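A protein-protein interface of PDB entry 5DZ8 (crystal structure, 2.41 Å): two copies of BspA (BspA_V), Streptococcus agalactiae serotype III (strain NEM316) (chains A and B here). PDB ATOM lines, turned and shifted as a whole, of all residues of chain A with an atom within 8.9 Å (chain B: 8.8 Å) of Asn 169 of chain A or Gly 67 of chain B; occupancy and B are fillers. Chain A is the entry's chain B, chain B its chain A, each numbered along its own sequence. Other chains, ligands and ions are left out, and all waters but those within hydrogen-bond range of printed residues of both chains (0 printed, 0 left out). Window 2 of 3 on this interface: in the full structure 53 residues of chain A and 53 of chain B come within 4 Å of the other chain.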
ATOM      1  N   VAL A 166      -9.218 -27.663  24.025  1.00  0.00           N
ATOM      2  CA  VAL A 166      -8.495 -28.859  23.634  1.00  0.00           C
ATOM      3  C   VAL A 166      -9.029 -29.280  22.274  1.00  0.00           C
ATOM      4  O   VAL A 166     -10.244 -29.384  22.051  1.00  0.00           O
ATOM      5  CB  VAL A 166      -8.656 -30.023  24.666  1.00  0.00           C
ATOM      6  CG1 VAL A 166      -7.822 -31.236  24.271  1.00  0.00           C
ATOM      7  CG2 VAL A 166      -8.294 -29.595  26.089  1.00  0.00           C
ATOM      8  N   ASN A 167      -8.116 -29.524  21.357  1.00  0.00           N
ATOM      9  CA  ASN A 167      -8.463 -30.153  20.091  1.00  0.00           C
ATOM     10  C   ASN A 167      -8.426 -31.698  20.264  1.00  0.00           C
ATOM     11  O   ASN A 167      -7.375 -32.307  20.336  1.00  0.00           O
ATOM     12  CB  ASN A 167      -7.500 -29.739  19.020  1.00  0.00           C
ATOM     13  CG  ASN A 167      -7.867 -30.277  17.680  1.00  0.00           C
ATOM     14  OD1 ASN A 167      -8.720 -31.173  17.550  1.00  0.00           O
ATOM     15  ND2 ASN A 167      -7.209 -29.765  16.655  1.00  0.00           N
ATOM     16  N   ASN A 168      -9.600 -32.290  20.321  1.00  0.00           N
ATOM     17  CA  ASN A 168      -9.759 -33.709  20.539  1.00  0.00           C
ATOM     18  C   ASN A 168      -9.560 -34.576  19.306  1.00  0.00           C
ATOM     19  O   ASN A 168      -9.664 -35.753  19.408  1.00  0.00           O
ATOM     20  CB  ASN A 168     -11.149 -33.965  21.126  1.00  0.00           C
ATOM     21  CG  ASN A 168     -11.302 -33.433  22.560  1.00  0.00           C
ATOM     22  OD1 ASN A 168     -12.384 -33.010  22.951  1.00  0.00           O
ATOM     23  ND2 ASN A 168     -10.251 -33.494  23.346  1.00  0.00           N
ATOM     24  N   ASN A 169      -9.238 -34.012  18.155  1.00  0.00           N
ATOM     25  CA  ASN A 169      -8.731 -34.834  17.067  1.00  0.00           C
ATOM     26  C   ASN A 169      -7.404 -35.524  17.436  1.00  0.00           C
ATOM     27  O   ASN A 169      -7.021 -36.514  16.783  1.00  0.00           O
ATOM     28  CB  ASN A 169      -8.493 -34.008  15.816  1.00  0.00           C
ATOM     29  CG  ASN A 169      -9.778 -33.563  15.131  1.00  0.00           C
ATOM     30  OD1 ASN A 169     -10.844 -34.164  15.281  1.00  0.00           O
ATOM     31  ND2 ASN A 169      -9.649 -32.525  14.300  1.00  0.00           N
ATOM     32  N   GLY B   1     -15.467 -30.588  10.382  1.00  0.00           N
ATOM     33  CA  GLY B   1     -15.541 -29.387  11.275  1.00  0.00           C
ATOM     34  C   GLY B   1     -14.982 -29.560  12.684  1.00  0.00           C
ATOM     35  O   GLY B   1     -14.595 -30.644  13.092  1.00  0.00           O
ATOM     36  N   PRO B   2     -14.942 -28.475  13.460  1.00  0.00           N
ATOM     37  CA  PRO B   2     -14.239 -28.595  14.734  1.00  0.00           C
ATOM     38  C   PRO B   2     -14.771 -29.731  15.566  1.00  0.00           C
ATOM     39  O   PRO B   2     -15.972 -29.909  15.772  1.00  0.00           O
ATOM     40  CB  PRO B   2     -14.523 -27.270  15.424  1.00  0.00           C
ATOM     41  CG  PRO B   2     -14.824 -26.331  14.298  1.00  0.00           C
ATOM     42  CD  PRO B   2     -15.557 -27.148  13.283  1.00  0.00           C
ATOM     43  N   ASN B   3     -13.745 -30.239  16.591  1.00  0.00           N
ATOM     44  CA  ASN B   3     -13.954 -31.186  17.618  1.00  0.00           C
ATOM     45  C   ASN B   3     -13.119 -30.657  18.804  1.00  0.00           C
ATOM     46  O   ASN B   3     -12.040 -31.152  19.110  1.00  0.00           O
ATOM     47  CB  ASN B   3     -13.505 -32.560  17.150  1.00  0.00           C
ATOM     48  CG  ASN B   3     -13.650 -33.559  18.242  1.00  0.00           C
ATOM     49  OD1 ASN B   3     -14.502 -33.385  19.099  1.00  0.00           O
ATOM     50  ND2 ASN B   3     -12.778 -34.540  18.293  1.00  0.00           N
ATOM     51  N   VAL B   4     -13.634 -29.590  19.401  1.00  0.00           N
ATOM     52  CA  VAL B   4     -13.007 -28.892  20.465  1.00  0.00           C
ATOM     53  C   VAL B   4     -13.745 -29.010  21.769  1.00  0.00           C
ATOM     54  O   VAL B   4     -14.873 -28.715  21.799  1.00  0.00           O
ATOM     55  CB  VAL B   4     -12.888 -27.409  20.143  1.00  0.00           C
ATOM     56  CG1 VAL B   4     -12.222 -26.705  21.337  1.00  0.00           C
ATOM     57  CG2 VAL B   4     -12.041 -27.223  18.882  1.00  0.00           C
ATOM     58  N   ALA B   5     -13.052 -29.375  22.847  1.00  0.00           N
ATOM     59  CA  ALA B   5     -13.603 -29.292  24.175  1.00  0.00           C
ATOM     60  C   ALA B   5     -13.249 -27.945  24.862  1.00  0.00           C
ATOM     61  O   ALA B   5     -12.063 -27.579  25.018  1.00  0.00           O
ATOM     62  CB  ALA B   5     -13.090 -30.469  24.989  1.00  0.00           C
ATOM     63  N   VAL B  62     -12.205 -22.268  13.609  1.00  0.00           N
ATOM     64  CA  VAL B  62     -12.010 -22.671  12.200  1.00  0.00           C
ATOM     65  C   VAL B  62     -11.288 -24.037  12.051  1.00  0.00           C
ATOM     66  O   VAL B  62     -10.160 -24.194  12.489  1.00  0.00           O
ATOM     67  CB  VAL B  62     -11.269 -21.573  11.406  1.00  0.00           C
ATOM     68  CG1 VAL B  62     -11.072 -22.000   9.946  1.00  0.00           C
ATOM     69  CG2 VAL B  62     -12.067 -20.267  11.472  1.00  0.00           C
ATOM     70  N   ALA B  63     -11.954 -25.032  11.465  1.00  0.00           N
ATOM     71  CA  ALA B  63     -11.293 -26.342  11.219  1.00  0.00           C
ATOM     72  C   ALA B  63     -10.343 -26.259  10.001  1.00  0.00           C
ATOM     73  O   ALA B  63     -10.683 -25.633   9.020  1.00  0.00           O
ATOM     74  CB  ALA B  63     -12.329 -27.420  11.006  1.00  0.00           C
ATOM     75  N   ASN B  64      -9.153 -26.846  10.079  1.00  0.00           N
ATOM     76  CA  ASN B  64      -8.263 -26.965   8.900  1.00  0.00           C
ATOM     77  C   ASN B  64      -8.261 -28.383   8.365  1.00  0.00           C
ATOM     78  O   ASN B  64      -8.645 -29.291   9.095  1.00  0.00           O
ATOM     79  CB  ASN B  64      -6.839 -26.559   9.254  1.00  0.00           C
ATOM     80  CG  ASN B  64      -6.774 -25.188   9.859  1.00  0.00           C
ATOM     81  OD1 ASN B  64      -7.321 -24.252   9.302  1.00  0.00           O
ATOM     82  ND2 ASN B  64      -6.096 -25.061  11.007  1.00  0.00           N
ATOM     83  N   LYS B  65      -7.809 -28.564   7.116  1.00  0.00           N
ATOM     84  CA  LYS B  65      -7.747 -29.891   6.446  1.00  0.00           C
ATOM     85  C   LYS B  65      -7.003 -30.960   7.257  1.00  0.00           C
ATOM     86  O   LYS B  65      -7.518 -32.043   7.479  1.00  0.00           O
ATOM     87  CB  LYS B  65      -7.071 -29.774   5.074  1.00  0.00           C
ATOM     88  N   ASP B  66      -5.822 -30.593   7.750  1.00  0.00           N
ATOM     89  CA  ASP B  66      -4.928 -31.482   8.534  1.00  0.00           C
ATOM     90  C   ASP B  66      -5.407 -31.897   9.942  1.00  0.00           C
ATOM     91  O   ASP B  66      -4.673 -32.558  10.679  1.00  0.00           O
ATOM     92  CB  ASP B  66      -3.571 -30.778   8.696  1.00  0.00           C
ATOM     93  CG  ASP B  66      -3.680 -29.496   9.504  1.00  0.00           C
ATOM     94  OD1 ASP B  66      -4.682 -29.342  10.219  1.00  0.00           O
ATOM     95  OD2 ASP B  66      -2.798 -28.620   9.407  1.00  0.00           O
ATOM     96  N   GLY B  67      -6.588 -31.435  10.352  1.00  0.00           N
ATOM     97  CA  GLY B  67      -7.154 -31.799  11.627  1.00  0.00           C
ATOM     98  C   GLY B  67      -6.874 -30.812  12.745  1.00  0.00           C
ATOM     99  O   GLY B  67      -7.450 -30.924  13.827  1.00  0.00           O
ATOM    100  N   SER B  68      -6.021 -29.844  12.482  1.00  0.00           N
ATOM    101  CA  SER B  68      -5.806 -28.758  13.427  1.00  0.00           C
ATOM    102  C   SER B  68      -7.017 -27.825  13.358  1.00  0.00           C
ATOM    103  O   SER B  68      -7.816 -27.877  12.412  1.00  0.00           O
ATOM    104  CB  SER B  68      -4.534 -28.018  13.082  1.00  0.00           C
ATOM    105  OG  SER B  68      -4.724 -27.279  11.897  1.00  0.00           O
ATOM    106  N   VAL B  69      -7.117 -26.964  14.364  1.00  0.00           N
ATOM    107  CA  VAL B  69      -8.187 -26.019  14.500  1.00  0.00           C
ATOM    108  C   VAL B  69      -7.639 -24.695  15.038  1.00  0.00           C
ATOM    109  O   VAL B  69      -6.611 -24.691  15.701  1.00  0.00           O
ATOM    110  CB  VAL B  69      -9.249 -26.588  15.426  1.00  0.00           C
ATOM    111  CG1 VAL B  69      -8.710 -26.681  16.876  1.00  0.00           C
ATOM    112  CG2 VAL B  69     -10.517 -25.737  15.371  1.00  0.00           C
ATOM    113  N   THR B  70      -8.277 -23.565  14.686  1.00  0.00           N
ATOM    114  CA  THR B  70      -7.937 -22.258  15.254  1.00  0.00           C
ATOM    115  C   THR B  70      -9.123 -21.833  16.101  1.00  0.00           C
ATOM    116  O   THR B  70     -10.266 -21.778  15.622  1.00  0.00           O
ATOM    117  CB  THR B  70      -7.661 -21.158  14.206  1.00  0.00           C
ATOM    118  OG1 THR B  70      -6.764 -21.612  13.195  1.00  0.00           O
ATOM    119  CG2 THR B  70      -7.025 -20.014  14.872  1.00  0.00           C
ATOM    120  N   LEU B 135      -4.333 -24.780  17.203  1.00  0.00           N
ATOM    121  CA  LEU B 135      -4.364 -26.049  17.930  1.00  0.00           C
ATOM    122  C   LEU B 135      -4.268 -27.265  17.011  1.00  0.00           C
ATOM    123  O   LEU B 135      -5.188 -27.601  16.297  1.00  0.00           O
ATOM    124  CB  LEU B 135      -5.618 -26.146  18.752  1.00  0.00           C
ATOM    125  CG  LEU B 135      -5.681 -25.722  20.225  1.00  0.00           C
ATOM    126  CD1 LEU B 135      -4.441 -25.118  20.893  1.00  0.00           C
ATOM    127  CD2 LEU B 135      -6.921 -24.869  20.358  1.00  0.00           C
ATOM    128  N   LYS B 136      -3.106 -27.888  17.064  1.00  0.00           N
ATOM    129  CA  LYS B 136      -2.847 -29.142  16.450  1.00  0.00           C
ATOM    130  C   LYS B 136      -3.683 -30.253  17.125  1.00  0.00           C
ATOM    131  O   LYS B 136      -4.126 -30.114  18.275  1.00  0.00           O
ATOM    132  CB  LYS B 136      -1.336 -29.481  16.623  1.00  0.00           C
ATOM    133  CG  LYS B 136      -0.506 -29.512  15.349  1.00  0.00           C
ATOM    134  CD  LYS B 136      -0.244 -28.144  14.826  1.00  0.00           C
ATOM    135  CE  LYS B 136       0.896 -28.158  13.819  1.00  0.00           C
ATOM    136  NZ  LYS B 136       0.564 -29.055  12.722  1.00  0.00           N
ATOM    137  N   PRO B 137      -3.837 -31.392  16.436  1.00  0.00           N
ATOM    138  CA  PRO B 137      -4.502 -32.533  17.051  1.00  0.00           C
ATOM    139  C   PRO B 137      -3.924 -32.847  18.425  1.00  0.00           C
ATOM    140  O   PRO B 137      -2.714 -32.926  18.590  1.00  0.00           O
ATOM    141  CB  PRO B 137      -4.257 -33.664  16.044  1.00  0.00           C
ATOM    142  CG  PRO B 137      -4.106 -32.945  14.703  1.00  0.00           C
ATOM    143  CD  PRO B 137      -3.386 -31.679  15.051  1.00  0.00           C
ATOM    144  N   HIS B 138      -4.817 -32.942  19.412  1.00  0.00           N
ATOM    145  CA  HIS B 138      -4.482 -33.147  20.796  1.00  0.00           C
ATOM    146  C   HIS B 138      -3.755 -31.985  21.471  1.00  0.00           C
ATOM    147  O   HIS B 138      -3.243 -32.171  22.568  1.00  0.00           O
ATOM    148  CB  HIS B 138      -3.720 -34.452  20.994  1.00  0.00           C
ATOM    149  CG  HIS B 138      -4.450 -35.656  20.505  1.00  0.00           C
ATOM    150  ND1 HIS B 138      -5.434 -36.279  21.243  1.00  0.00           N
ATOM    151  CD2 HIS B 138      -4.349 -36.350  19.345  1.00  0.00           C
ATOM    152  CE1 HIS B 138      -5.892 -37.320  20.568  1.00  0.00           C
ATOM    153  NE2 HIS B 138      -5.242 -37.389  19.418  1.00  0.00           N
ATOM    154  N   ALA B 139      -3.729 -30.794  20.862  1.00  0.00           N
ATOM    155  CA  ALA B 139      -3.166 -29.657  21.538  1.00  0.00           C
ATOM    156  C   ALA B 139      -4.200 -29.057  22.504  1.00  0.00           C
ATOM    157  O   ALA B 139      -5.411 -29.203  22.359  1.00  0.00           O
ATOM    158  CB  ALA B 139      -2.708 -28.639  20.540  1.00  0.00           C
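O of Asn 3 of chain B sits at hydrogen-bond distance from N of Asn 168 of chain A, at 3.0 Å. The backbone NH (N) of Ala 5 of chain B sits at hydrogen-bond distance from the backbone carbonyl oxygen (O) of Val 166 of chain A (2.9 Å). The backbone carbonyl oxygen of Gly 67 of chain B is in hydrogen-bond range of the side-chain amide nitrogen of Asn 167 of chain A (3.1 Å). ND2 of Asn 169 of chain A sits at hydrogen-bond distance from O of Gly 67 of chain B (2.8 Å). The backbone carbonyl oxygen (O) of Leu 135 of chain B lies within hydrogen-bond range of the side-chain amide nitrogen (ND2) of Asn 167 of chain A, at 3.0 Å. O of Lys 136 of chain B sits close to ND2 of Asn 167 of chain A, at 3.5 Å. N of His 138 of chain B is in hydrogen-bond range of O of Asn 167 of chain A, 2.8 Å away. NE2 of His 138 of chain B is in hydrogen-bond range of O of Asn 169 of chain A. O of Ala 139 of chain B lies within hydrogen-bond range of N of Asn 167 of chain A, at 2.9 Å.
The side-chain hydroxyl of Ser 68 of chain B is in hydrogen-bond range of the side-chain amide nitrogen of Asn 64 of chain B (2.8 Å). OD1 of Asp 66 of chain B is in hydrogen-bond range of OG of Ser 68 of chain B (2.7 Å). N of Leu 135 of chain B lies within hydrogen-bond range of O of Val 69 of chain B (2.7 Å). OD1 of Asn 167 of chain A sits at hydrogen-bond distance from N of Asn 169 of chain A, 2.9 Å away.
Asn 3 of chain B touches Val 166 of chain A. Val 166 of chain A touches Val 4 of chain B. Ala 139 of chain B touches Val 166 of chain A (O to CA, 3.4 Å). Asn 3 of chain B touches Asn 167 of chain A (O to OD1, 3.7 Å). Asn 167 of chain A touches Ser 68 of chain B. Val 69 of chain B touches Asn 167 of chain A. Asn 167 of chain A touches Pro 137 of chain B (ND2 to N, 3.8 Å). Asn 168 of chain A touches Ala 5 of chain B. Asn 169 of chain A touches Asn 3 of chain B. Asn 169 of chain A touches Pro 137 of chain B.
Printed residues of chain B within 4 Å of Asn 167 of chain A: Asn 3, Gly 67, Ser 68, Val 69, Leu 135, Lys 136, Pro 137, His 138 and Ala 139. Printed residues of chain B within 4 Å of Asn 169 of chain A: Asn 3 (3.6 Å), Gly 67 (2.8 Å), Pro 137 (3.9 Å) and His 138 (3.3 Å). Pro 2 of chain B touches none of the printed residues of chain A. Of chain A, only Asn 167 (3.1 Å) and Asn 169 (2.8 Å) come within 4 Å of Gly 67 of chain B. Ser 68 of chain B touches just one residue of chain A: Asn 167 (3.7 Å). Thr 70 of chain B touches none of the printed residues of chain A. Printed residues of chain A within 4 Å of Leu 135 of chain B: Asn 167. Of the printed residues of chain A, Lys 136 of chain B touches Asn 167. The nearest residue of chain B that does not touch Asn 169 of chain A is Ser 68 of chain B (4.9 Å). The nearest residue of chain A that does not touch Gly 67 of chain B is Asn 168 of chain A (6.9 Å). The nearest printed residue of chain A that does not touch Val 69 of chain B is Val 166 of chain A (6.0 Å).
Of the 4 printed residues of chain A, 4 touch a printed residue of chain B. Hydrophobic or aromatic side chains of chain A within 4 Å of the printed part of chain B: Val 166. Printed residues of chain B that touch a printed residue of chain A: Asn 3, Val 4, Ala 5, Gly 67, Ser 68, Val 69, Leu 135, Lys 136, Pro 137, His 138 and Ala 139. Hydrophobic or aromatic side chains of chain B that line the printed part of chain A: Val 4, Ala 5, Val 69, Pro 137 and His 138. Among the printed residues, no Asp or Glu carboxylate lies within 4 Å of a Lys or Arg side-chain nitrogen of the other chain.
No position is printed for both chains.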
